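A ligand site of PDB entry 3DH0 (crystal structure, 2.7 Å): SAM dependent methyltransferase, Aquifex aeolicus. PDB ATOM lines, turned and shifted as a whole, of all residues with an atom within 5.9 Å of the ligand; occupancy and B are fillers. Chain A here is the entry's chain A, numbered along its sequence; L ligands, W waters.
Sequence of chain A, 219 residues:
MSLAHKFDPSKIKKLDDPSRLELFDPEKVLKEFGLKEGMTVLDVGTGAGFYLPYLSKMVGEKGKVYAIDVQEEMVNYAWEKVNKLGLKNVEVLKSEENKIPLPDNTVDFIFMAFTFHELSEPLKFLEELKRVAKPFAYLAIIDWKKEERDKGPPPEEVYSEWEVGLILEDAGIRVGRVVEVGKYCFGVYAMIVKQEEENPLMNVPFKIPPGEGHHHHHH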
ATOM      1  N   LYS A   6     -23.549  30.384  12.643  1.00  0.00           N
ATOM      2  CA  LYS A   6     -22.283  30.590  13.433  1.00  0.00           C
ATOM      3  C   LYS A   6     -22.411  31.773  14.376  1.00  0.00           C
ATOM      4  O   LYS A   6     -23.083  32.753  14.073  1.00  0.00           O
ATOM      5  CB  LYS A   6     -21.097  30.827  12.496  1.00  0.00           C
ATOM      6  CG  LYS A   6     -20.797  29.700  11.531  1.00  0.00           C
ATOM      7  CD  LYS A   6     -20.536  28.350  12.208  1.00  0.00           C
ATOM      8  CE  LYS A   6     -20.366  27.275  11.132  1.00  0.00           C
ATOM      9  NZ  LYS A   6     -20.344  25.901  11.644  1.00  0.00           N
ATOM     10  N   PHE A   7     -21.752  31.711  15.518  1.00  0.00           N
ATOM     11  CA  PHE A   7     -21.854  32.829  16.442  1.00  0.00           C
ATOM     12  C   PHE A   7     -21.198  34.040  15.803  1.00  0.00           C
ATOM     13  O   PHE A   7     -20.252  33.899  15.045  1.00  0.00           O
ATOM     14  CB  PHE A   7     -21.171  32.531  17.769  1.00  0.00           C
ATOM     15  CG  PHE A   7     -21.619  33.435  18.859  1.00  0.00           C
ATOM     16  CD1 PHE A   7     -22.813  33.186  19.532  1.00  0.00           C
ATOM     17  CD2 PHE A   7     -20.893  34.568  19.179  1.00  0.00           C
ATOM     18  CE1 PHE A   7     -23.271  34.044  20.506  1.00  0.00           C
ATOM     19  CE2 PHE A   7     -21.355  35.447  20.160  1.00  0.00           C
ATOM     20  CZ  PHE A   7     -22.545  35.185  20.833  1.00  0.00           C
ATOM     21  N   LEU A  15     -19.822  36.027  25.280  1.00  0.00           N
ATOM     22  CA  LEU A  15     -19.355  34.699  25.627  1.00  0.00           C
ATOM     23  C   LEU A  15     -18.371  34.771  26.794  1.00  0.00           C
ATOM     24  O   LEU A  15     -18.148  33.790  27.503  1.00  0.00           O
ATOM     25  CB  LEU A  15     -18.693  34.064  24.412  1.00  0.00           C
ATOM     26  CG  LEU A  15     -19.571  33.920  23.149  1.00  0.00           C
ATOM     27  CD1 LEU A  15     -18.710  33.486  21.954  1.00  0.00           C
ATOM     28  CD2 LEU A  15     -20.697  32.929  23.419  1.00  0.00           C
ATOM     29  N   ASP A  16     -17.801  35.947  27.017  1.00  0.00           N
ATOM     30  CA  ASP A  16     -16.831  36.159  28.081  1.00  0.00           C
ATOM     31  C   ASP A  16     -17.490  36.955  29.213  1.00  0.00           C
ATOM     32  O   ASP A  16     -16.948  37.942  29.711  1.00  0.00           O
ATOM     33  CB  ASP A  16     -15.614  36.912  27.508  1.00  0.00           C
ATOM     34  CG  ASP A  16     -14.353  36.694  28.305  1.00  0.00           C
ATOM     35  OD1 ASP A  16     -14.282  35.687  29.046  1.00  0.00           O
ATOM     36  OD2 ASP A  16     -13.412  37.516  28.194  1.00  0.00           O
ATOM     37  N   ARG A  20     -22.508  34.073  33.096  1.00  0.00           N
ATOM     38  CA  ARG A  20     -22.903  32.835  32.430  1.00  0.00           C
ATOM     39  C   ARG A  20     -22.939  31.752  33.491  1.00  0.00           C
ATOM     40  O   ARG A  20     -23.575  30.724  33.317  1.00  0.00           O
ATOM     41  CB  ARG A  20     -21.886  32.411  31.348  1.00  0.00           C
ATOM     42  CG  ARG A  20     -21.600  33.399  30.218  1.00  0.00           C
ATOM     43  CD  ARG A  20     -22.503  33.215  28.989  1.00  0.00           C
ATOM     44  NE  ARG A  20     -22.417  31.913  28.302  1.00  0.00           N
ATOM     45  CZ  ARG A  20     -21.350  31.406  27.686  1.00  0.00           C
ATOM     46  NH1 ARG A  20     -20.201  32.062  27.641  1.00  0.00           N
ATOM     47  NH2 ARG A  20     -21.454  30.244  27.055  1.00  0.00           N
ATOM     48  N   ASP A  43     -12.399  20.843  23.537  1.00  0.00           N
ATOM     49  CA  ASP A  43     -13.433  21.853  23.752  1.00  0.00           C
ATOM     50  C   ASP A  43     -13.774  22.323  22.355  1.00  0.00           C
ATOM     51  O   ASP A  43     -13.060  23.132  21.784  1.00  0.00           O
ATOM     52  CB  ASP A  43     -12.857  22.995  24.591  1.00  0.00           C
ATOM     53  CG  ASP A  43     -13.912  24.008  25.008  1.00  0.00           C
ATOM     54  OD1 ASP A  43     -15.114  23.720  24.884  1.00  0.00           O
ATOM     55  OD2 ASP A  43     -13.513  25.108  25.479  1.00  0.00           O
ATOM     56  N   VAL A  44     -14.880  21.831  21.810  1.00  0.00           N
ATOM     57  CA  VAL A  44     -15.279  22.159  20.448  1.00  0.00           C
ATOM     58  C   VAL A  44     -15.517  23.639  20.098  1.00  0.00           C
ATOM     59  O   VAL A  44     -14.691  24.243  19.416  1.00  0.00           O
ATOM     60  CB  VAL A  44     -16.469  21.280  20.031  1.00  0.00           C
ATOM     61  CG1 VAL A  44     -16.876  21.568  18.608  1.00  0.00           C
ATOM     62  CG2 VAL A  44     -16.057  19.824  20.148  1.00  0.00           C
ATOM     63  N   GLY A  45     -16.619  24.235  20.517  1.00  0.00           N
ATOM     64  CA  GLY A  45     -16.776  25.646  20.177  1.00  0.00           C
ATOM     65  C   GLY A  45     -16.170  26.477  21.291  1.00  0.00           C
ATOM     66  O   GLY A  45     -16.887  27.078  22.100  1.00  0.00           O
ATOM     67  N   THR A  46     -14.848  26.509  21.348  1.00  0.00           N
ATOM     68  CA  THR A  46     -14.169  27.232  22.410  1.00  0.00           C
ATOM     69  C   THR A  46     -14.584  28.697  22.533  1.00  0.00           C
ATOM     70  O   THR A  46     -14.573  29.257  23.626  1.00  0.00           O
ATOM     71  CB  THR A  46     -12.659  27.104  22.264  1.00  0.00           C
ATOM     72  OG1 THR A  46     -12.050  27.284  23.544  1.00  0.00           O
ATOM     73  CG2 THR A  46     -12.119  28.159  21.309  1.00  0.00           C
ATOM     74  N   GLY A  47     -14.935  29.315  21.412  1.00  0.00           N
ATOM     75  CA  GLY A  47     -15.358  30.712  21.430  1.00  0.00           C
ATOM     76  C   GLY A  47     -14.411  31.685  22.104  1.00  0.00           C
ATOM     77  O   GLY A  47     -13.300  31.914  21.636  1.00  0.00           O
ATOM     78  N   ALA A  48     -14.852  32.275  23.209  1.00  0.00           N
ATOM     79  CA  ALA A  48     -14.027  33.210  23.941  1.00  0.00           C
ATOM     80  C   ALA A  48     -13.076  32.483  24.894  1.00  0.00           C
ATOM     81  O   ALA A  48     -12.142  33.055  25.424  1.00  0.00           O
ATOM     82  CB  ALA A  48     -14.921  34.176  24.725  1.00  0.00           C
ATOM     83  N   GLY A  49     -13.331  31.188  25.092  1.00  0.00           N
ATOM     84  CA  GLY A  49     -12.509  30.392  25.984  1.00  0.00           C
ATOM     85  C   GLY A  49     -12.995  30.522  27.409  1.00  0.00           C
ATOM     86  O   GLY A  49     -12.222  30.371  28.349  1.00  0.00           O
ATOM     87  N   PHE A  50     -14.289  30.805  27.551  1.00  0.00           N
ATOM     88  CA  PHE A  50     -14.922  31.005  28.845  1.00  0.00           C
ATOM     89  C   PHE A  50     -14.736  29.847  29.799  1.00  0.00           C
ATOM     90  O   PHE A  50     -14.238  30.036  30.910  1.00  0.00           O
ATOM     91  CB  PHE A  50     -16.414  31.282  28.671  1.00  0.00           C
ATOM     92  CG  PHE A  50     -17.118  31.568  29.963  1.00  0.00           C
ATOM     93  CD1 PHE A  50     -16.846  32.745  30.668  1.00  0.00           C
ATOM     94  CD2 PHE A  50     -18.019  30.661  30.499  1.00  0.00           C
ATOM     95  CE1 PHE A  50     -17.467  33.003  31.892  1.00  0.00           C
ATOM     96  CE2 PHE A  50     -18.638  30.897  31.734  1.00  0.00           C
ATOM     97  CZ  PHE A  50     -18.359  32.069  32.428  1.00  0.00           C
ATOM     98  N   TYR A  51     -15.140  28.645  29.403  1.00  0.00           N
ATOM     99  CA  TYR A  51     -14.995  27.474  30.252  1.00  0.00           C
ATOM    100  C   TYR A  51     -13.574  26.894  30.310  1.00  0.00           C
ATOM    101  O   TYR A  51     -13.327  25.930  31.028  1.00  0.00           O
ATOM    102  CB  TYR A  51     -15.965  26.390  29.807  1.00  0.00           C
ATOM    103  CG  TYR A  51     -17.409  26.760  30.001  1.00  0.00           C
ATOM    104  CD1 TYR A  51     -17.933  26.909  31.282  1.00  0.00           C
ATOM    105  CD2 TYR A  51     -18.240  26.983  28.918  1.00  0.00           C
ATOM    106  CE1 TYR A  51     -19.259  27.285  31.472  1.00  0.00           C
ATOM    107  CE2 TYR A  51     -19.580  27.361  29.107  1.00  0.00           C
ATOM    108  CZ  TYR A  51     -20.069  27.508  30.387  1.00  0.00           C
ATOM    109  OH  TYR A  51     -21.359  27.890  30.582  1.00  0.00           O
ATOM    110  N   ILE A  68     -10.579  24.138  20.169  1.00  0.00           N
ATOM    111  CA  ILE A  68     -10.727  24.468  18.762  1.00  0.00           C
ATOM    112  C   ILE A  68     -11.860  25.437  18.491  1.00  0.00           C
ATOM    113  O   ILE A  68     -12.642  25.756  19.362  1.00  0.00           O
ATOM    114  CB  ILE A  68     -10.963  23.210  17.916  1.00  0.00           C
ATOM    115  CG1 ILE A  68     -12.167  22.439  18.477  1.00  0.00           C
ATOM    116  CG2 ILE A  68      -9.704  22.354  17.884  1.00  0.00           C
ATOM    117  CD1 ILE A  68     -12.606  21.257  17.641  1.00  0.00           C
ATOM    118  N   ASP A  69     -11.939  25.902  17.259  1.00  0.00           N
ATOM    119  CA  ASP A  69     -12.964  26.823  16.846  1.00  0.00           C
ATOM    120  C   ASP A  69     -12.725  27.190  15.402  1.00  0.00           C
ATOM    121  O   ASP A  69     -11.615  27.554  15.024  1.00  0.00           O
ATOM    122  CB  ASP A  69     -12.956  28.073  17.711  1.00  0.00           C
ATOM    123  CG  ASP A  69     -14.290  28.804  17.697  1.00  0.00           C
ATOM    124  OD1 ASP A  69     -14.787  29.113  16.602  1.00  0.00           O
ATOM    125  OD2 ASP A  69     -14.849  29.050  18.788  1.00  0.00           O
ATOM    126  N   VAL A  70     -13.773  27.095  14.581  1.00  0.00           N
ATOM    127  CA  VAL A  70     -13.706  27.407  13.158  1.00  0.00           C
ATOM    128  C   VAL A  70     -13.425  28.872  12.864  1.00  0.00           C
ATOM    129  O   VAL A  70     -12.934  29.181  11.790  1.00  0.00           O
ATOM    130  CB  VAL A  70     -15.014  27.041  12.422  1.00  0.00           C
ATOM    131  CG1 VAL A  70     -15.207  25.532  12.369  1.00  0.00           C
ATOM    132  CG2 VAL A  70     -16.194  27.723  13.106  1.00  0.00           C
ATOM    133  N   GLN A  71     -13.749  29.765  13.799  1.00  0.00           N
ATOM    134  CA  GLN A  71     -13.512  31.191  13.572  1.00  0.00           C
ATOM    135  C   GLN A  71     -12.193  31.708  14.127  1.00  0.00           C
ATOM    136  O   GLN A  71     -11.900  31.563  15.313  1.00  0.00           O
ATOM    137  CB  GLN A  71     -14.678  32.009  14.091  1.00  0.00           C
ATOM    138  CG  GLN A  71     -15.937  31.791  13.283  1.00  0.00           C
ATOM    139  CD  GLN A  71     -17.012  32.814  13.565  1.00  0.00           C
ATOM    140  OE1 GLN A  71     -17.790  32.675  14.499  1.00  0.00           O
ATOM    141  NE2 GLN A  71     -17.045  33.867  12.750  1.00  0.00           N
ATOM    142  N   MET A  74     -12.256  34.068  17.137  1.00  0.00           N
ATOM    143  CA  MET A  74     -12.488  33.383  18.398  1.00  0.00           C
ATOM    144  C   MET A  74     -11.212  32.666  18.837  1.00  0.00           C
ATOM    145  O   MET A  74     -10.899  32.597  20.025  1.00  0.00           O
ATOM    146  CB  MET A  74     -13.630  32.371  18.257  1.00  0.00           C
ATOM    147  CG  MET A  74     -15.003  32.937  18.601  1.00  0.00           C
ATOM    148  SD  MET A  74     -15.623  34.122  17.427  1.00  0.00           S
ATOM    149  CE  MET A  74     -17.326  33.789  17.519  1.00  0.00           C
ATOM    150  N   SER A  95      -9.759  25.479  13.870  1.00  0.00           N
ATOM    151  CA  SER A  95     -10.479  24.346  13.300  1.00  0.00           C
ATOM    152  C   SER A  95     -11.192  24.648  11.987  1.00  0.00           C
ATOM    153  O   SER A  95     -11.405  25.806  11.612  1.00  0.00           O
ATOM    154  CB  SER A  95     -11.488  23.826  14.338  1.00  0.00           C
ATOM    155  OG  SER A  95     -12.532  23.048  13.753  1.00  0.00           O
ATOM    156  N   GLU A  96     -11.547  23.576  11.290  1.00  0.00           N
ATOM    157  CA  GLU A  96     -12.252  23.662  10.015  1.00  0.00           C
ATOM    158  C   GLU A  96     -13.571  22.961  10.287  1.00  0.00           C
ATOM    159  O   GLU A  96     -13.634  22.083  11.137  1.00  0.00           O
ATOM    160  CB  GLU A  96     -11.470  22.932   8.931  1.00  0.00           C
ATOM    161  CG  GLU A  96     -11.458  23.629   7.586  1.00  0.00           C
ATOM    162  CD  GLU A  96     -10.779  24.985   7.629  1.00  0.00           C
ATOM    163  OE1 GLU A  96      -9.776  25.141   8.367  1.00  0.00           O
ATOM    164  OE2 GLU A  96     -11.239  25.893   6.923  1.00  0.00           O
ATOM    165  N   GLU A  97     -14.619  23.323   9.561  1.00  0.00           N
ATOM    166  CA  GLU A  97     -15.940  22.743   9.783  1.00  0.00           C
ATOM    167  C   GLU A  97     -16.014  21.276  10.166  1.00  0.00           C
ATOM    168  O   GLU A  97     -16.538  20.941  11.229  1.00  0.00           O
ATOM    169  CB  GLU A  97     -16.827  23.024   8.575  1.00  0.00           C
ATOM    170  CG  GLU A  97     -18.319  22.743   8.801  1.00  0.00           C
ATOM    171  CD  GLU A  97     -18.903  23.505   9.982  1.00  0.00           C
ATOM    172  OE1 GLU A  97     -18.578  24.698  10.164  1.00  0.00           O
ATOM    173  OE2 GLU A  97     -19.712  22.906  10.718  1.00  0.00           O
ATOM    174  N   ASN A  98     -15.502  20.375   9.347  1.00  0.00           N
ATOM    175  CA  ASN A  98     -15.595  18.954   9.708  1.00  0.00           C
ATOM    176  C   ASN A  98     -14.250  18.255   9.807  1.00  0.00           C
ATOM    177  O   ASN A  98     -14.171  17.038   9.596  1.00  0.00           O
ATOM    178  CB  ASN A  98     -16.480  18.214   8.719  1.00  0.00           C
ATOM    179  CG  ASN A  98     -17.868  18.829   8.615  1.00  0.00           C
ATOM    180  OD1 ASN A  98     -18.173  19.514   7.644  1.00  0.00           O
ATOM    181  ND2 ASN A  98     -18.695  18.580   9.623  1.00  0.00           N
ATOM    182  N   ALA A 113     -19.972  22.729  24.534  1.00  0.00           N
ATOM    183  CA  ALA A 113     -20.882  23.661  25.203  1.00  0.00           C
ATOM    184  C   ALA A 113     -21.536  24.699  24.300  1.00  0.00           C
ATOM    185  O   ALA A 113     -20.884  25.634  23.835  1.00  0.00           O
ATOM    186  CB  ALA A 113     -20.161  24.353  26.361  1.00  0.00           C
ATOM    187  N   PHE A 114     -22.835  24.544  24.092  1.00  0.00           N
ATOM    188  CA  PHE A 114     -23.621  25.449  23.253  1.00  0.00           C
ATOM    189  C   PHE A 114     -23.126  25.564  21.817  1.00  0.00           C
ATOM    190  O   PHE A 114     -23.342  26.576  21.164  1.00  0.00           O
ATOM    191  CB  PHE A 114     -23.667  26.850  23.864  1.00  0.00           C
ATOM    192  CG  PHE A 114     -24.203  26.886  25.265  1.00  0.00           C
ATOM    193  CD1 PHE A 114     -23.343  27.058  26.342  1.00  0.00           C
ATOM    194  CD2 PHE A 114     -25.566  26.728  25.503  1.00  0.00           C
ATOM    195  CE1 PHE A 114     -23.827  27.086  27.637  1.00  0.00           C
ATOM    196  CE2 PHE A 114     -26.063  26.751  26.791  1.00  0.00           C
ATOM    197  CZ  PHE A 114     -25.194  26.933  27.870  1.00  0.00           C
ATOM    198  N   THR A 115     -22.487  24.513  21.317  1.00  0.00           N
ATOM    199  CA  THR A 115     -21.993  24.588  19.960  1.00  0.00           C
ATOM    200  C   THR A 115     -22.589  23.554  19.010  1.00  0.00           C
ATOM    201  O   THR A 115     -22.513  23.714  17.782  1.00  0.00           O
ATOM    202  CB  THR A 115     -20.409  24.521  19.967  1.00  0.00           C
ATOM    203  OG1 THR A 115     -19.909  24.183  18.664  1.00  0.00           O
ATOM    204  CG2 THR A 115     -19.926  23.516  20.973  1.00  0.00           C
ATOM    205  N   HIS A 117     -25.738  22.833  18.080  1.00  0.00           N
ATOM    206  CA  HIS A 117     -26.733  23.377  17.162  1.00  0.00           C
ATOM    207  C   HIS A 117     -26.131  24.321  16.114  1.00  0.00           C
ATOM    208  O   HIS A 117     -26.838  24.797  15.232  1.00  0.00           O
ATOM    209  CB  HIS A 117     -27.807  24.149  17.946  1.00  0.00           C
ATOM    210  CG  HIS A 117     -27.301  25.406  18.562  1.00  0.00           C
ATOM    211  ND1 HIS A 117     -26.490  25.408  19.674  1.00  0.00           N
ATOM    212  CD2 HIS A 117     -27.408  26.701  18.168  1.00  0.00           C
ATOM    213  CE1 HIS A 117     -26.106  26.651  19.931  1.00  0.00           C
ATOM    214  NE2 HIS A 117     -26.653  27.449  19.038  1.00  0.00           N
ATOM    215  N   GLU A 118     -24.833  24.599  16.208  1.00  0.00           N
ATOM    216  CA  GLU A 118     -24.166  25.483  15.257  1.00  0.00           C
ATOM    217  C   GLU A 118     -23.420  24.741  14.144  1.00  0.00           C
ATOM    218  O   GLU A 118     -22.896  25.353  13.205  1.00  0.00           O
ATOM    219  CB  GLU A 118     -23.178  26.402  15.991  1.00  0.00           C
ATOM    220  CG  GLU A 118     -23.740  27.731  16.384  1.00  0.00           C
ATOM    221  CD  GLU A 118     -22.668  28.695  16.822  1.00  0.00           C
ATOM    222  OE1 GLU A 118     -21.661  28.839  16.108  1.00  0.00           O
ATOM    223  OE2 GLU A 118     -22.836  29.326  17.881  1.00  0.00           O
ATOM    224  N   LEU A 119     -23.352  23.415  14.251  1.00  0.00           N
ATOM    225  CA  LEU A 119     -22.661  22.605  13.273  1.00  0.00           C
ATOM    226  C   LEU A 119     -23.357  22.522  11.901  1.00  0.00           C
ATOM    227  O   LEU A 119     -24.518  22.129  11.822  1.00  0.00           O
ATOM    228  CB  LEU A 119     -22.484  21.189  13.819  1.00  0.00           C
ATOM    229  CG  LEU A 119     -21.745  21.047  15.158  1.00  0.00           C
ATOM    230  CD1 LEU A 119     -21.821  19.607  15.665  1.00  0.00           C
ATOM    231  CD2 LEU A 119     -20.302  21.482  14.970  1.00  0.00           C
ATOM    232  N   SER A 120     -22.640  22.891  10.841  1.00  0.00           N
ATOM    233  CA  SER A 120     -23.208  22.810   9.485  1.00  0.00           C
ATOM    234  C   SER A 120     -23.672  21.381   9.194  1.00  0.00           C
ATOM    235  O   SER A 120     -24.828  21.137   8.858  1.00  0.00           O
ATOM    236  CB  SER A 120     -22.174  23.228   8.443  1.00  0.00           C
ATOM    237  OG  SER A 120     -21.908  24.619   8.503  1.00  0.00           O
ATOM    238  N   PHE A 125     -19.561  15.688  11.209  1.00  0.00           N
ATOM    239  CA  PHE A 125     -18.631  16.234  12.192  1.00  0.00           C
ATOM    240  C   PHE A 125     -18.420  15.152  13.241  1.00  0.00           C
ATOM    241  O   PHE A 125     -17.297  14.943  13.730  1.00  0.00           O
ATOM    242  CB  PHE A 125     -19.206  17.479  12.828  1.00  0.00           C
ATOM    243  CG  PHE A 125     -18.348  18.049  13.913  1.00  0.00           C
ATOM    244  CD1 PHE A 125     -18.508  17.637  15.231  1.00  0.00           C
ATOM    245  CD2 PHE A 125     -17.347  18.965  13.605  1.00  0.00           C
ATOM    246  CE1 PHE A 125     -17.682  18.130  16.226  1.00  0.00           C
ATOM    247  CE2 PHE A 125     -16.513  19.468  14.602  1.00  0.00           C
ATOM    248  CZ  PHE A 125     -16.679  19.055  15.907  1.00  0.00           C
HETATM  249  N1  LIG L   1     -18.756  27.364  24.201  1.00  0.00           N
HETATM  250  C1  LIG L   1     -18.418  28.819  24.303  1.00  0.00           C
HETATM  251  C2  LIG L   1     -18.567  29.298  25.727  1.00  0.00           C
HETATM  252  O1  LIG L   1     -18.928  28.491  26.586  1.00  0.00           O
HETATM  253  O2  LIG L   1     -18.300  30.537  25.923  1.00  0.00           O
HETATM  254  C3  LIG L   1     -19.346  29.620  23.399  1.00  0.00           C
HETATM  255  C4  LIG L   1     -19.447  28.941  22.083  1.00  0.00           C
HETATM  256  S1  LIG L   1     -20.479  29.638  20.768  1.00  0.00           S
HETATM  257  C5  LIG L   1     -22.151  29.358  21.387  1.00  0.00           C
HETATM  258  C6  LIG L   1     -20.234  28.445  19.530  1.00  0.00           C
HETATM  259  C7  LIG L   1     -18.892  28.492  18.833  1.00  0.00           C
HETATM  260  O3  LIG L   1     -18.913  27.389  17.936  1.00  0.00           O
HETATM  261  C8  LIG L   1     -18.745  29.697  17.882  1.00  0.00           C
HETATM  262  O4  LIG L   1     -17.714  30.529  18.481  1.00  0.00           O
HETATM  263  C9  LIG L   1     -18.206  29.132  16.581  1.00  0.00           C
HETATM  264  O5  LIG L   1     -17.134  29.796  15.927  1.00  0.00           O
HETATM  265  C10 LIG L   1     -17.996  27.634  16.956  1.00  0.00           C
HETATM  266  N2  LIG L   1     -18.237  26.641  15.934  1.00  0.00           N
HETATM  267  C11 LIG L   1     -19.272  26.522  15.032  1.00  0.00           C
HETATM  268  N3  LIG L   1     -19.168  25.477  14.270  1.00  0.00           N
HETATM  269  C12 LIG L   1     -17.986  24.862  14.676  1.00  0.00           C
HETATM  270  C13 LIG L   1     -17.312  23.688  14.242  1.00  0.00           C
HETATM  271  N4  LIG L   1     -17.790  22.916  13.248  1.00  0.00           N
HETATM  272  N5  LIG L   1     -16.119  23.350  14.877  1.00  0.00           N
HETATM  273  C14 LIG L   1     -15.678  24.153  15.870  1.00  0.00           C
HETATM  274  N6  LIG L   1     -16.245  25.269  16.347  1.00  0.00           N
HETATM  275  C15 LIG L   1     -17.398  25.575  15.697  1.00  0.00           C
HETATM  276  O   HOH W   1     -16.483  25.965  25.706  1.00  0.00           O
HETATM  277  O   HOH W   2     -15.982  31.309  25.351  1.00  0.00           O
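OD1 of Asp 69 is in hydrogen-bond range of O5 of the ligand, 2.5 Å away.
A nitrogen (N1) of the ligand is in hydrogen-bond range of the backbone carbonyl oxygen (O) of Ala 113 (2.8 Å).
O of Gly 45 is in hydrogen-bond range of N1 of the ligand, at 2.8 Å.
N3 of the ligand sits at hydrogen-bond distance from NZ of Lys 6, at 2.9 Å.
The guanidinium group of Arg 20 is in salt-bridge range of an oxygen (O2) of the ligand (3.0 Å).
N4 of the ligand sits at hydrogen-bond distance from O of Glu 97 (3.1 Å).
The side-chain carboxylate (OE2) of Glu 97 is in hydrogen-bond range of a nitrogen (N4) of the ligand (3.2 Å).
OE1 of Gln 71 is in hydrogen-bond range of O5 of the ligand (3.3 Å).
An oxygen (O3) of the ligand lies within hydrogen-bond range of the side-chain hydroxyl of Thr 115 (3.4 Å).
Water W1 lies within hydrogen-bond range of the side-chain carboxylate of Asp 43 and a nitrogen (N1) of the ligand.
The side-chain carboxylate (OD1) of Asp 69 sits at hydrogen-bond distance from the backbone NH (N) of Gln 71.
OE1 of Glu 97 lies within salt-bridge range of NZ of Lys 6.
NH1 of Arg 20 lies within hydrogen-bond range of O of Leu 15 (2.7 Å).
The side-chain amide oxygen of Gln 71 lies close to the backbone carbonyl oxygen of Phe 7.
The backbone carbonyl oxygen (O) of Val 44 lies close to the backbone carbonyl oxygen (O) of Ile 68 (2.5 Å).
The side-chain amide nitrogen (ND2) of Asn 98 sits close to the backbone NH (N) of Phe 125, at 3.4 Å.
N of Thr 46 lies within hydrogen-bond range of O of Ile 68 (3.1 Å).
OD2 of Asp 43 is in hydrogen-bond range of OG1 of Thr 46.
OE2 of Glu 118 sits close to S1 of the ligand.
Merely in contact with the ligand: Phe 7 (3.7 Å), Leu 15 (3.6 Å), Val 44 (3.6 Å), Thr 46 (3.9 Å), Gly 47 (3.8 Å), Phe 50 (3.4 Å), Tyr 51 (2.8 Å), Val 70 (3.4 Å), Met 74 (3.4 Å), Ser 95 (3.8 Å), Phe 114 (3.0 Å), Leu 119 (3.4 Å) and Phe 125 (3.9 Å).
Hydrophobic or aromatic side chains within 4 Å of the ligand: Phe 7, Leu 15, Val 44, Phe 50, Tyr 51, Val 70, Met 74, Ala 113, Phe 114, Leu 119 and Phe 125.
Within 4 Å of the ligand: Lys 6, Phe 7, Leu 15, Arg 20, Val 44, Gly 45, Thr 46, Gly 47, Phe 50, Tyr 51, Asp 69, Val 70, Gln 71, Met 74, Ser 95, Glu 97, Ala 113, Phe 114, Thr 115, Glu 118, Leu 119 and Phe 125.
The nearest printed residue that does not touch the ligand is Ile 68 (4.6 Å).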
